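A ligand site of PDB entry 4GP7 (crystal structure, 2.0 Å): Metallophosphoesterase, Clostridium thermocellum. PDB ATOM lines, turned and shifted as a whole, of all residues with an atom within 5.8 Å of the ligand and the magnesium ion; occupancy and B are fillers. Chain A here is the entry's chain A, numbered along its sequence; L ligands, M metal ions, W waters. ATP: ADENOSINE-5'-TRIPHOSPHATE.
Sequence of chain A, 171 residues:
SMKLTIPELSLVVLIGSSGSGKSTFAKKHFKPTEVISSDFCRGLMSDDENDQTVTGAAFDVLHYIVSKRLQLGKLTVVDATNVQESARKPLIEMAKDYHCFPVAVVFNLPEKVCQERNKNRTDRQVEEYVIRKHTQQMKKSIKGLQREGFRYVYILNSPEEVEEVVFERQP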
ATOM      1  N   GLY A  16      -4.451  24.298 -19.254  1.00  0.00           N
ATOM      2  CA  GLY A  16      -4.202  24.427 -20.681  1.00  0.00           C
ATOM      3  C   GLY A  16      -4.772  25.698 -21.270  1.00  0.00           C
ATOM      4  O   GLY A  16      -5.726  26.291 -20.736  1.00  0.00           O
ATOM      5  N   SER A  17      -4.172  26.122 -22.368  1.00  0.00           N
ATOM      6  CA  SER A  17      -4.620  27.282 -23.114  1.00  0.00           C
ATOM      7  C   SER A  17      -6.094  27.206 -23.491  1.00  0.00           C
ATOM      8  O   SER A  17      -6.684  26.131 -23.535  1.00  0.00           O
ATOM      9  CB  SER A  17      -3.797  27.401 -24.392  1.00  0.00           C
ATOM     10  OG  SER A  17      -4.306  28.418 -25.237  1.00  0.00           O
ATOM     11  N   SER A  18      -6.672  28.358 -23.798  1.00  0.00           N
ATOM     12  CA  SER A  18      -7.951  28.351 -24.494  1.00  0.00           C
ATOM     13  C   SER A  18      -7.781  27.554 -25.788  1.00  0.00           C
ATOM     14  O   SER A  18      -6.773  27.684 -26.481  1.00  0.00           O
ATOM     15  CB  SER A  18      -8.398  29.764 -24.844  1.00  0.00           C
ATOM     16  OG  SER A  18      -9.624  29.694 -25.537  1.00  0.00           O
ATOM     17  N   GLY A  19      -8.758  26.719 -26.110  1.00  0.00           N
ATOM     18  CA  GLY A  19      -8.687  25.910 -27.311  1.00  0.00           C
ATOM     19  C   GLY A  19      -7.954  24.589 -27.121  1.00  0.00           C
ATOM     20  O   GLY A  19      -7.931  23.762 -28.031  1.00  0.00           O
ATOM     21  N   SER A  20      -7.362  24.361 -25.937  1.00  0.00           N
ATOM     22  CA  SER A  20      -6.616  23.121 -25.730  1.00  0.00           C
ATOM     23  C   SER A  20      -7.505  21.872 -25.526  1.00  0.00           C
ATOM     24  O   SER A  20      -7.007  20.756 -25.421  1.00  0.00           O
ATOM     25  CB  SER A  20      -5.600  23.269 -24.577  1.00  0.00           C
ATOM     26  OG  SER A  20      -6.267  23.377 -23.334  1.00  0.00           O
ATOM     27  N   GLY A  21      -8.823  22.066 -25.460  1.00  0.00           N
ATOM     28  CA  GLY A  21      -9.742  20.935 -25.389  1.00  0.00           C
ATOM     29  C   GLY A  21     -10.128  20.479 -23.982  1.00  0.00           C
ATOM     30  O   GLY A  21     -10.660  19.372 -23.796  1.00  0.00           O
ATOM     31  N   LYS A  22      -9.895  21.336 -23.003  1.00  0.00           N
ATOM     32  CA  LYS A  22     -10.184  21.017 -21.601  1.00  0.00           C
ATOM     33  C   LYS A  22     -11.624  20.617 -21.364  1.00  0.00           C
ATOM     34  O   LYS A  22     -11.889  19.591 -20.721  1.00  0.00           O
ATOM     35  CB  LYS A  22      -9.826  22.202 -20.694  1.00  0.00           C
ATOM     36  CG  LYS A  22      -8.365  22.611 -20.760  1.00  0.00           C
ATOM     37  CD  LYS A  22      -8.084  23.694 -19.753  1.00  0.00           C
ATOM     38  CE  LYS A  22      -8.944  24.930 -20.021  1.00  0.00           C
ATOM     39  NZ  LYS A  22      -8.648  25.553 -21.341  1.00  0.00           N
ATOM     40  N   SER A  23     -12.566  21.414 -21.861  1.00  0.00           N
ATOM     41  CA  SER A  23     -13.986  21.170 -21.589  1.00  0.00           C
ATOM     42  C   SER A  23     -14.472  19.915 -22.301  1.00  0.00           C
ATOM     43  O   SER A  23     -15.349  19.198 -21.806  1.00  0.00           O
ATOM     44  CB  SER A  23     -14.835  22.381 -21.993  1.00  0.00           C
ATOM     45  OG  SER A  23     -14.541  23.503 -21.174  1.00  0.00           O
ATOM     46  N   THR A  24     -13.905  19.657 -23.472  1.00  0.00           N
ATOM     47  CA  THR A  24     -14.195  18.462 -24.250  1.00  0.00           C
ATOM     48  C   THR A  24     -13.729  17.232 -23.489  1.00  0.00           C
ATOM     49  O   THR A  24     -14.474  16.276 -23.262  1.00  0.00           O
ATOM     50  CB  THR A  24     -13.467  18.526 -25.598  1.00  0.00           C
ATOM     51  OG1 THR A  24     -13.908  19.691 -26.316  1.00  0.00           O
ATOM     52  CG2 THR A  24     -13.740  17.288 -26.438  1.00  0.00           C
ATOM     53  N   PHE A  25     -12.477  17.281 -23.064  1.00  0.00           N
ATOM     54  CA  PHE A  25     -11.865  16.231 -22.266  1.00  0.00           C
ATOM     55  C   PHE A  25     -12.700  16.003 -21.000  1.00  0.00           C
ATOM     56  O   PHE A  25     -12.971  14.856 -20.624  1.00  0.00           O
ATOM     57  CB  PHE A  25     -10.431  16.655 -21.947  1.00  0.00           C
ATOM     58  CG  PHE A  25      -9.647  15.695 -21.097  1.00  0.00           C
ATOM     59  CD1 PHE A  25      -9.788  15.691 -19.709  1.00  0.00           C
ATOM     60  CD2 PHE A  25      -8.717  14.846 -21.672  1.00  0.00           C
ATOM     61  CE1 PHE A  25      -9.034  14.836 -18.917  1.00  0.00           C
ATOM     62  CE2 PHE A  25      -7.958  13.983 -20.890  1.00  0.00           C
ATOM     63  CZ  PHE A  25      -8.115  13.979 -19.508  1.00  0.00           C
ATOM     64  N   ASP A  79     -12.421  23.128 -14.457  1.00  0.00           N
ATOM     65  CA  ASP A  79     -12.255  23.356 -15.873  1.00  0.00           C
ATOM     66  C   ASP A  79     -12.083  24.849 -16.101  1.00  0.00           C
ATOM     67  O   ASP A  79     -13.036  25.593 -16.304  1.00  0.00           O
ATOM     68  CB  ASP A  79     -13.468  22.815 -16.619  1.00  0.00           C
ATOM     69  CG  ASP A  79     -13.375  23.026 -18.106  1.00  0.00           C
ATOM     70  OD1 ASP A  79     -12.259  23.314 -18.590  1.00  0.00           O
ATOM     71  OD2 ASP A  79     -14.410  22.903 -18.794  1.00  0.00           O
ATOM     72  N   ALA A  80     -10.833  25.285 -16.035  1.00  0.00           N
ATOM     73  CA  ALA A  80     -10.473  26.672 -16.293  1.00  0.00           C
ATOM     74  C   ALA A  80      -9.069  26.621 -16.856  1.00  0.00           C
ATOM     75  O   ALA A  80      -8.455  25.553 -16.887  1.00  0.00           O
ATOM     76  CB  ALA A  80     -10.498  27.457 -15.008  1.00  0.00           C
ATOM     77  N   THR A  81      -8.557  27.749 -17.312  1.00  0.00           N
ATOM     78  CA  THR A  81      -7.248  27.785 -17.954  1.00  0.00           C
ATOM     79  C   THR A  81      -6.150  27.310 -16.990  1.00  0.00           C
ATOM     80  O   THR A  81      -5.331  26.460 -17.342  1.00  0.00           O
ATOM     81  CB  THR A  81      -6.891  29.207 -18.479  1.00  0.00           C
ATOM     82  OG1 THR A  81      -6.926  30.155 -17.413  1.00  0.00           O
ATOM     83  CG2 THR A  81      -7.900  29.638 -19.515  1.00  0.00           C
ATOM     84  N   ARG A 117      -7.811  25.043 -33.305  1.00  0.00           N
ATOM     85  CA  ARG A 117      -9.114  24.664 -32.774  1.00  0.00           C
ATOM     86  C   ARG A 117      -9.945  25.901 -32.461  1.00  0.00           C
ATOM     87  O   ARG A 117     -11.153  25.904 -32.664  1.00  0.00           O
ATOM     88  CB  ARG A 117      -8.956  23.782 -31.551  1.00  0.00           C
ATOM     89  CG  ARG A 117      -8.342  22.448 -31.870  1.00  0.00           C
ATOM     90  CD  ARG A 117      -8.044  21.724 -30.604  1.00  0.00           C
ATOM     91  NE  ARG A 117      -7.406  20.443 -30.844  1.00  0.00           N
ATOM     92  CZ  ARG A 117      -7.136  19.581 -29.866  1.00  0.00           C
ATOM     93  NH1 ARG A 117      -7.459  19.898 -28.617  1.00  0.00           N
ATOM     94  NH2 ARG A 117      -6.554  18.431 -30.129  1.00  0.00           N
ATOM     95  N   ASN A 118      -9.272  26.940 -32.006  1.00  0.00           N
ATOM     96  CA  ASN A 118      -9.923  28.214 -31.709  1.00  0.00           C
ATOM     97  C   ASN A 118     -10.737  28.744 -32.890  1.00  0.00           C
ATOM     98  O   ASN A 118     -11.889  29.141 -32.723  1.00  0.00           O
ATOM     99  CB  ASN A 118      -8.869  29.239 -31.310  1.00  0.00           C
ATOM    100  CG  ASN A 118      -9.454  30.599 -30.971  1.00  0.00           C
ATOM    101  OD1 ASN A 118     -10.328  30.702 -30.109  1.00  0.00           O
ATOM    102  ND2 ASN A 118      -8.962  31.641 -31.641  1.00  0.00           N
ATOM    103  N   ASN A 120     -12.063  27.324 -35.288  1.00  0.00           N
ATOM    104  CA  ASN A 120     -13.178  26.512 -35.730  1.00  0.00           C
ATOM    105  C   ASN A 120     -14.265  26.379 -34.677  1.00  0.00           C
ATOM    106  O   ASN A 120     -15.239  25.640 -34.866  1.00  0.00           O
ATOM    107  CB  ASN A 120     -12.659  25.174 -36.274  1.00  0.00           C
ATOM    108  CG  ASN A 120     -11.626  25.376 -37.394  1.00  0.00           C
ATOM    109  OD1 ASN A 120     -11.993  25.702 -38.520  1.00  0.00           O
ATOM    110  ND2 ASN A 120     -10.343  25.218 -37.076  1.00  0.00           N
ATOM    111  N   ARG A 121     -14.125  27.128 -33.582  1.00  0.00           N
ATOM    112  CA  ARG A 121     -15.108  27.108 -32.502  1.00  0.00           C
ATOM    113  C   ARG A 121     -16.375  27.836 -32.874  1.00  0.00           C
ATOM    114  O   ARG A 121     -16.337  28.939 -33.439  1.00  0.00           O
ATOM    115  CB  ARG A 121     -14.547  27.748 -31.221  1.00  0.00           C
ATOM    116  CG  ARG A 121     -13.344  27.043 -30.666  1.00  0.00           C
ATOM    117  CD  ARG A 121     -12.938  27.636 -29.333  1.00  0.00           C
ATOM    118  NE  ARG A 121     -13.959  27.459 -28.304  1.00  0.00           N
ATOM    119  CZ  ARG A 121     -13.719  27.588 -27.004  1.00  0.00           C
ATOM    120  NH1 ARG A 121     -12.494  27.892 -26.586  1.00  0.00           N
ATOM    121  NH2 ARG A 121     -14.689  27.412 -26.127  1.00  0.00           N
ATOM    122  N   THR A 122     -17.490  27.241 -32.494  1.00  0.00           N
ATOM    123  CA  THR A 122     -18.802  27.791 -32.807  1.00  0.00           C
ATOM    124  C   THR A 122     -19.378  28.483 -31.588  1.00  0.00           C
ATOM    125  O   THR A 122     -20.349  29.239 -31.703  1.00  0.00           O
ATOM    126  CB  THR A 122     -19.756  26.674 -33.264  1.00  0.00           C
ATOM    127  OG1 THR A 122     -20.001  25.771 -32.182  1.00  0.00           O
ATOM    128  CG2 THR A 122     -19.128  25.912 -34.425  1.00  0.00           C
ATOM    129  N   ASP A 123     -18.772  28.259 -30.431  1.00  0.00           N
ATOM    130  CA  ASP A 123     -19.263  28.863 -29.193  1.00  0.00           C
ATOM    131  C   ASP A 123     -18.659  30.244 -28.944  1.00  0.00           C
ATOM    132  O   ASP A 123     -19.386  31.230 -28.816  1.00  0.00           O
ATOM    133  CB  ASP A 123     -19.087  27.930 -27.979  1.00  0.00           C
ATOM    134  CG  ASP A 123     -17.677  27.350 -27.859  1.00  0.00           C
ATOM    135  OD1 ASP A 123     -16.943  27.287 -28.876  1.00  0.00           O
ATOM    136  OD2 ASP A 123     -17.313  26.908 -26.737  1.00  0.00           O
ATOM    137  N   ARG A 124     -17.339  30.312 -28.868  1.00  0.00           N
ATOM    138  CA  ARG A 124     -16.652  31.587 -28.680  1.00  0.00           C
ATOM    139  C   ARG A 124     -15.197  31.437 -29.087  1.00  0.00           C
ATOM    140  O   ARG A 124     -14.659  30.320 -29.099  1.00  0.00           O
ATOM    141  CB  ARG A 124     -16.743  32.029 -27.222  1.00  0.00           C
ATOM    142  CG  ARG A 124     -16.159  31.027 -26.275  1.00  0.00           C
ATOM    143  CD  ARG A 124     -16.460  31.336 -24.821  1.00  0.00           C
ATOM    144  NE  ARG A 124     -16.159  30.175 -24.000  1.00  0.00           N
ATOM    145  CZ  ARG A 124     -14.925  29.774 -23.686  1.00  0.00           C
ATOM    146  NH1 ARG A 124     -13.875  30.478 -24.093  1.00  0.00           N
ATOM    147  NH2 ARG A 124     -14.752  28.684 -22.953  1.00  0.00           N
ATOM    148  N   VAL A 126     -11.108  33.478 -29.227  1.00  0.00           N
ATOM    149  CA  VAL A 126     -10.265  34.510 -28.642  1.00  0.00           C
ATOM    150  C   VAL A 126      -9.254  34.958 -29.674  1.00  0.00           C
ATOM    151  O   VAL A 126      -9.044  34.286 -30.683  1.00  0.00           O
ATOM    152  CB  VAL A 126      -9.553  33.991 -27.358  1.00  0.00           C
ATOM    153  CG1 VAL A 126     -10.570  33.603 -26.301  1.00  0.00           C
ATOM    154  CG2 VAL A 126      -8.661  32.814 -27.666  1.00  0.00           C
ATOM    155  N   PRO A 159      -2.142  15.527 -29.156  1.00  0.00           N
ATOM    156  CA  PRO A 159      -3.540  15.091 -29.252  1.00  0.00           C
ATOM    157  C   PRO A 159      -3.727  13.584 -29.123  1.00  0.00           C
ATOM    158  O   PRO A 159      -4.701  13.136 -28.522  1.00  0.00           O
ATOM    159  CB  PRO A 159      -3.947  15.572 -30.651  1.00  0.00           C
ATOM    160  CG  PRO A 159      -3.184  16.831 -30.810  1.00  0.00           C
ATOM    161  CD  PRO A 159      -1.833  16.564 -30.150  1.00  0.00           C
ATOM    162  N   VAL A 162      -3.626  12.716 -25.592  1.00  0.00           N
ATOM    163  CA  VAL A 162      -4.892  13.151 -25.008  1.00  0.00           C
ATOM    164  C   VAL A 162      -6.005  12.170 -25.332  1.00  0.00           C
ATOM    165  O   VAL A 162      -6.829  11.831 -24.475  1.00  0.00           O
ATOM    166  CB  VAL A 162      -5.274  14.553 -25.513  1.00  0.00           C
ATOM    167  CG1 VAL A 162      -6.687  14.873 -25.122  1.00  0.00           C
ATOM    168  CG2 VAL A 162      -4.305  15.602 -24.977  1.00  0.00           C
ATOM    169  N   GLU A 163      -6.025  11.684 -26.562  1.00  0.00           N
ATOM    170  CA  GLU A 163      -7.049  10.706 -26.987  1.00  0.00           C
ATOM    171  C   GLU A 163      -6.954   9.382 -26.230  1.00  0.00           C
ATOM    172  O   GLU A 163      -7.976   8.784 -25.888  1.00  0.00           O
ATOM    173  CB  GLU A 163      -6.925  10.457 -28.492  1.00  0.00           C
ATOM    174  CG  GLU A 163      -8.119  10.925 -29.280  1.00  0.00           C
ATOM    175  CD  GLU A 163      -9.397  10.198 -28.897  1.00  0.00           C
ATOM    176  OE1 GLU A 163      -9.377   8.952 -28.886  1.00  0.00           O
ATOM    177  OE2 GLU A 163     -10.392  10.882 -28.585  1.00  0.00           O
HETATM  178  PG  ATP L   1     -11.549  27.350 -23.108  1.00  0.00           P
HETATM  179  O1G ATP L   1     -11.566  28.523 -24.045  1.00  0.00           O
HETATM  180  O2G ATP L   1     -10.394  27.449 -22.135  1.00  0.00           O
HETATM  181  O3G ATP L   1     -12.858  26.939 -22.497  1.00  0.00           O
HETATM  182  PB  ATP L   1     -11.111  24.585 -23.848  1.00  0.00           P
HETATM  183  O1B ATP L   1     -12.300  24.187 -23.001  1.00  0.00           O
HETATM  184  O2B ATP L   1      -9.703  24.175 -23.468  1.00  0.00           O
HETATM  185  O3B ATP L   1     -11.125  26.173 -24.140  1.00  0.00           O
HETATM  186  PA  ATP L   1     -12.663  23.186 -25.783  1.00  0.00           P
HETATM  187  O1A ATP L   1     -13.844  24.118 -25.819  1.00  0.00           O
HETATM  188  O2A ATP L   1     -12.832  21.885 -25.025  1.00  0.00           O
HETATM  189  O3A ATP L   1     -11.355  24.031 -25.339  1.00  0.00           O
HETATM  190  O5' ATP L   1     -12.229  22.906 -27.312  1.00  0.00           O
HETATM  191  C5' ATP L   1     -12.091  24.026 -28.193  1.00  0.00           C
HETATM  192  C4' ATP L   1     -12.474  23.607 -29.609  1.00  0.00           C
HETATM  193  O4' ATP L   1     -11.558  22.602 -30.074  1.00  0.00           O
HETATM  194  C3' ATP L   1     -13.868  22.995 -29.630  1.00  0.00           C
HETATM  195  O3' ATP L   1     -14.574  23.445 -30.789  1.00  0.00           O
HETATM  196  C2' ATP L   1     -13.613  21.506 -29.759  1.00  0.00           C
HETATM  197  O2' ATP L   1     -14.659  20.827 -30.450  1.00  0.00           O
HETATM  198  C1' ATP L   1     -12.264  21.407 -30.457  1.00  0.00           C
HETATM  199  N9  ATP L   1     -11.602  20.193 -29.934  1.00  0.00           N
HETATM  200  C8  ATP L   1     -11.639  19.815 -28.650  1.00  0.00           C
HETATM  201  N7  ATP L   1     -10.970  18.642 -28.461  1.00  0.00           N
HETATM  202  C5  ATP L   1     -10.508  18.257 -29.658  1.00  0.00           C
HETATM  203  C6  ATP L   1      -9.722  17.101 -30.158  1.00  0.00           C
HETATM  204  N6  ATP L   1      -9.310  16.141 -29.293  1.00  0.00           N
HETATM  205  N1  ATP L   1      -9.437  17.053 -31.476  1.00  0.00           N
HETATM  206  C2  ATP L   1      -9.858  18.030 -32.320  1.00  0.00           C
HETATM  207  N3  ATP L   1     -10.575  19.100 -31.933  1.00  0.00           N
HETATM  208  C4  ATP L   1     -10.937  19.273 -30.631  1.00  0.00           C
HETATM  209 MG    MG M   1     -13.705  25.217 -21.944  1.00  0.00          MG
HETATM  210  O   HOH W   1      -9.736  17.036 -25.675  1.00  0.00           O
HETATM  211  O   HOH W   2     -14.894  25.188 -23.620  1.00  0.00           O
HETATM  212  O   HOH W   3      -7.495  14.244 -28.897  1.00  0.00           O
HETATM  213  O   HOH W   4     -16.112  24.079 -27.230  1.00  0.00           O
HETATM  214  O   HOH W   5     -12.920  23.880 -32.724  1.00  0.00           O
HETATM  215  O   HOH W   6     -12.530  25.395 -20.221  1.00  0.00           O
HETATM  216  O   HOH W   7      -9.350  13.380 -27.579  1.00  0.00           O
HETATM  217  O   HOH W   8     -11.307  27.721 -19.518  1.00  0.00           O
HETATM  218  O   HOH W   9     -15.072  26.326 -20.783  1.00  0.00           O
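An oxygen (O2A) of the ligand lies within hydrogen-bond range of the backbone NH (N) of Ser 23 (3.2 Å). The guanidinium group (NH1) of Arg 124 lies within salt-bridge range of an oxygen (O1G) of the ligand (3.0 Å). N of Lys 22 sits at hydrogen-bond distance from O2B of the ligand (2.9 Å). An oxygen (O2G) of the ligand is in salt-bridge range of the side-chain amino group (NZ) of Lys 22 (2.7 Å). The side-chain hydroxyl of Ser 18 lies within hydrogen-bond range of an oxygen (O1G) of the ligand (2.7 Å). The backbone NH of Thr 24 sits at hydrogen-bond distance from an oxygen (O2A) of the ligand (2.9 Å). The side-chain hydroxyl (OG1) of Thr 24 sits at hydrogen-bond distance from an oxygen (O2A) of the ligand (2.8 Å). An oxygen (O1G) of the ligand is in salt-bridge range of the guanidinium group (NH1) of Arg 121. N of Gly 21 is in hydrogen-bond range of O2B of the ligand (3.0 Å). The backbone NH of Gly 19 lies within hydrogen-bond range of an oxygen (O3B) of the ligand, at 3.1 Å. The guanidinium group of Arg 117 sits close to a nitrogen (N1) of the ligand, 3.5 Å away. An oxygen (O2B) of the ligand is in hydrogen-bond range of the backbone NH of Ser 20.
The side-chain carboxylate of Asp 79 lies close to the side-chain hydroxyl of Ser 23 (2.5 Å). O of Arg 124 is in hydrogen-bond range of NE of Arg 121. The side-chain amino group (NZ) of Lys 22 sits at hydrogen-bond distance from the backbone carbonyl oxygen (O) of Ser 17, 3.0 Å away. The backbone carbonyl oxygen (O) of Gly 16 is in hydrogen-bond range of the side-chain amino group (NZ) of Lys 22 (3.1 Å). The guanidinium group of Arg 121 is in salt-bridge range of the side-chain carboxylate of Asp 123, 2.7 Å away. O of Ser 20 is in hydrogen-bond range of NH1 of Arg 117, at 3.3 Å. O of Ser 17 lies within hydrogen-bond range of OG of Ser 20.
Ser 17 touches the ligand (O to O2B, 3.6 Å). Of the 24 residues printed, 11 come within 4 Å of the ligand. Along chain A the residues within 4 Å of the ligand span positions 17 to 124. The nearest printed residue that does not touch the ligand is Thr 81 (4.2 Å).
Merely in contact with the magnesium ion: Asp 79 and Arg 124. Of the 24 residues printed, 3 come within 4 Å of the magnesium ion.
The magnesium ion is bound by an oxygen (O3G) of the ligand (2.0 Å), an oxygen (O1B) of the ligand (2.0 Å), water W2 (2.1 Å), the side-chain hydroxyl (OG) of Ser 23 (2.1 Å), water W6 (2.1 Å) and water W9 (2.1 Å). The magnesium ion has six donor atoms within binding distance.
Water W2 bridges O1A of the ligand and NH2 of Arg 121. Water W5 bridges an oxygen (O3') of the ligand (2.6 Å) and the backbone carbonyl oxygen (O) of Arg 117 (2.7 Å). Water W3 bridges N6 of the ligand and O of Pro 159. Water W4 bridges O1A of the ligand (2.7 Å) and OD2 of Asp 123 (3.1 Å). Water W7 lies within hydrogen-bond range of the side-chain carboxylate (OE2) of Glu 163 (2.9 Å) and a nitrogen (N6) of the ligand (3.3 Å). Water W1 bridges the backbone carbonyl oxygen of Gly 21 (3.1 Å) and a nitrogen (N7) of the ligand (3.4 Å).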
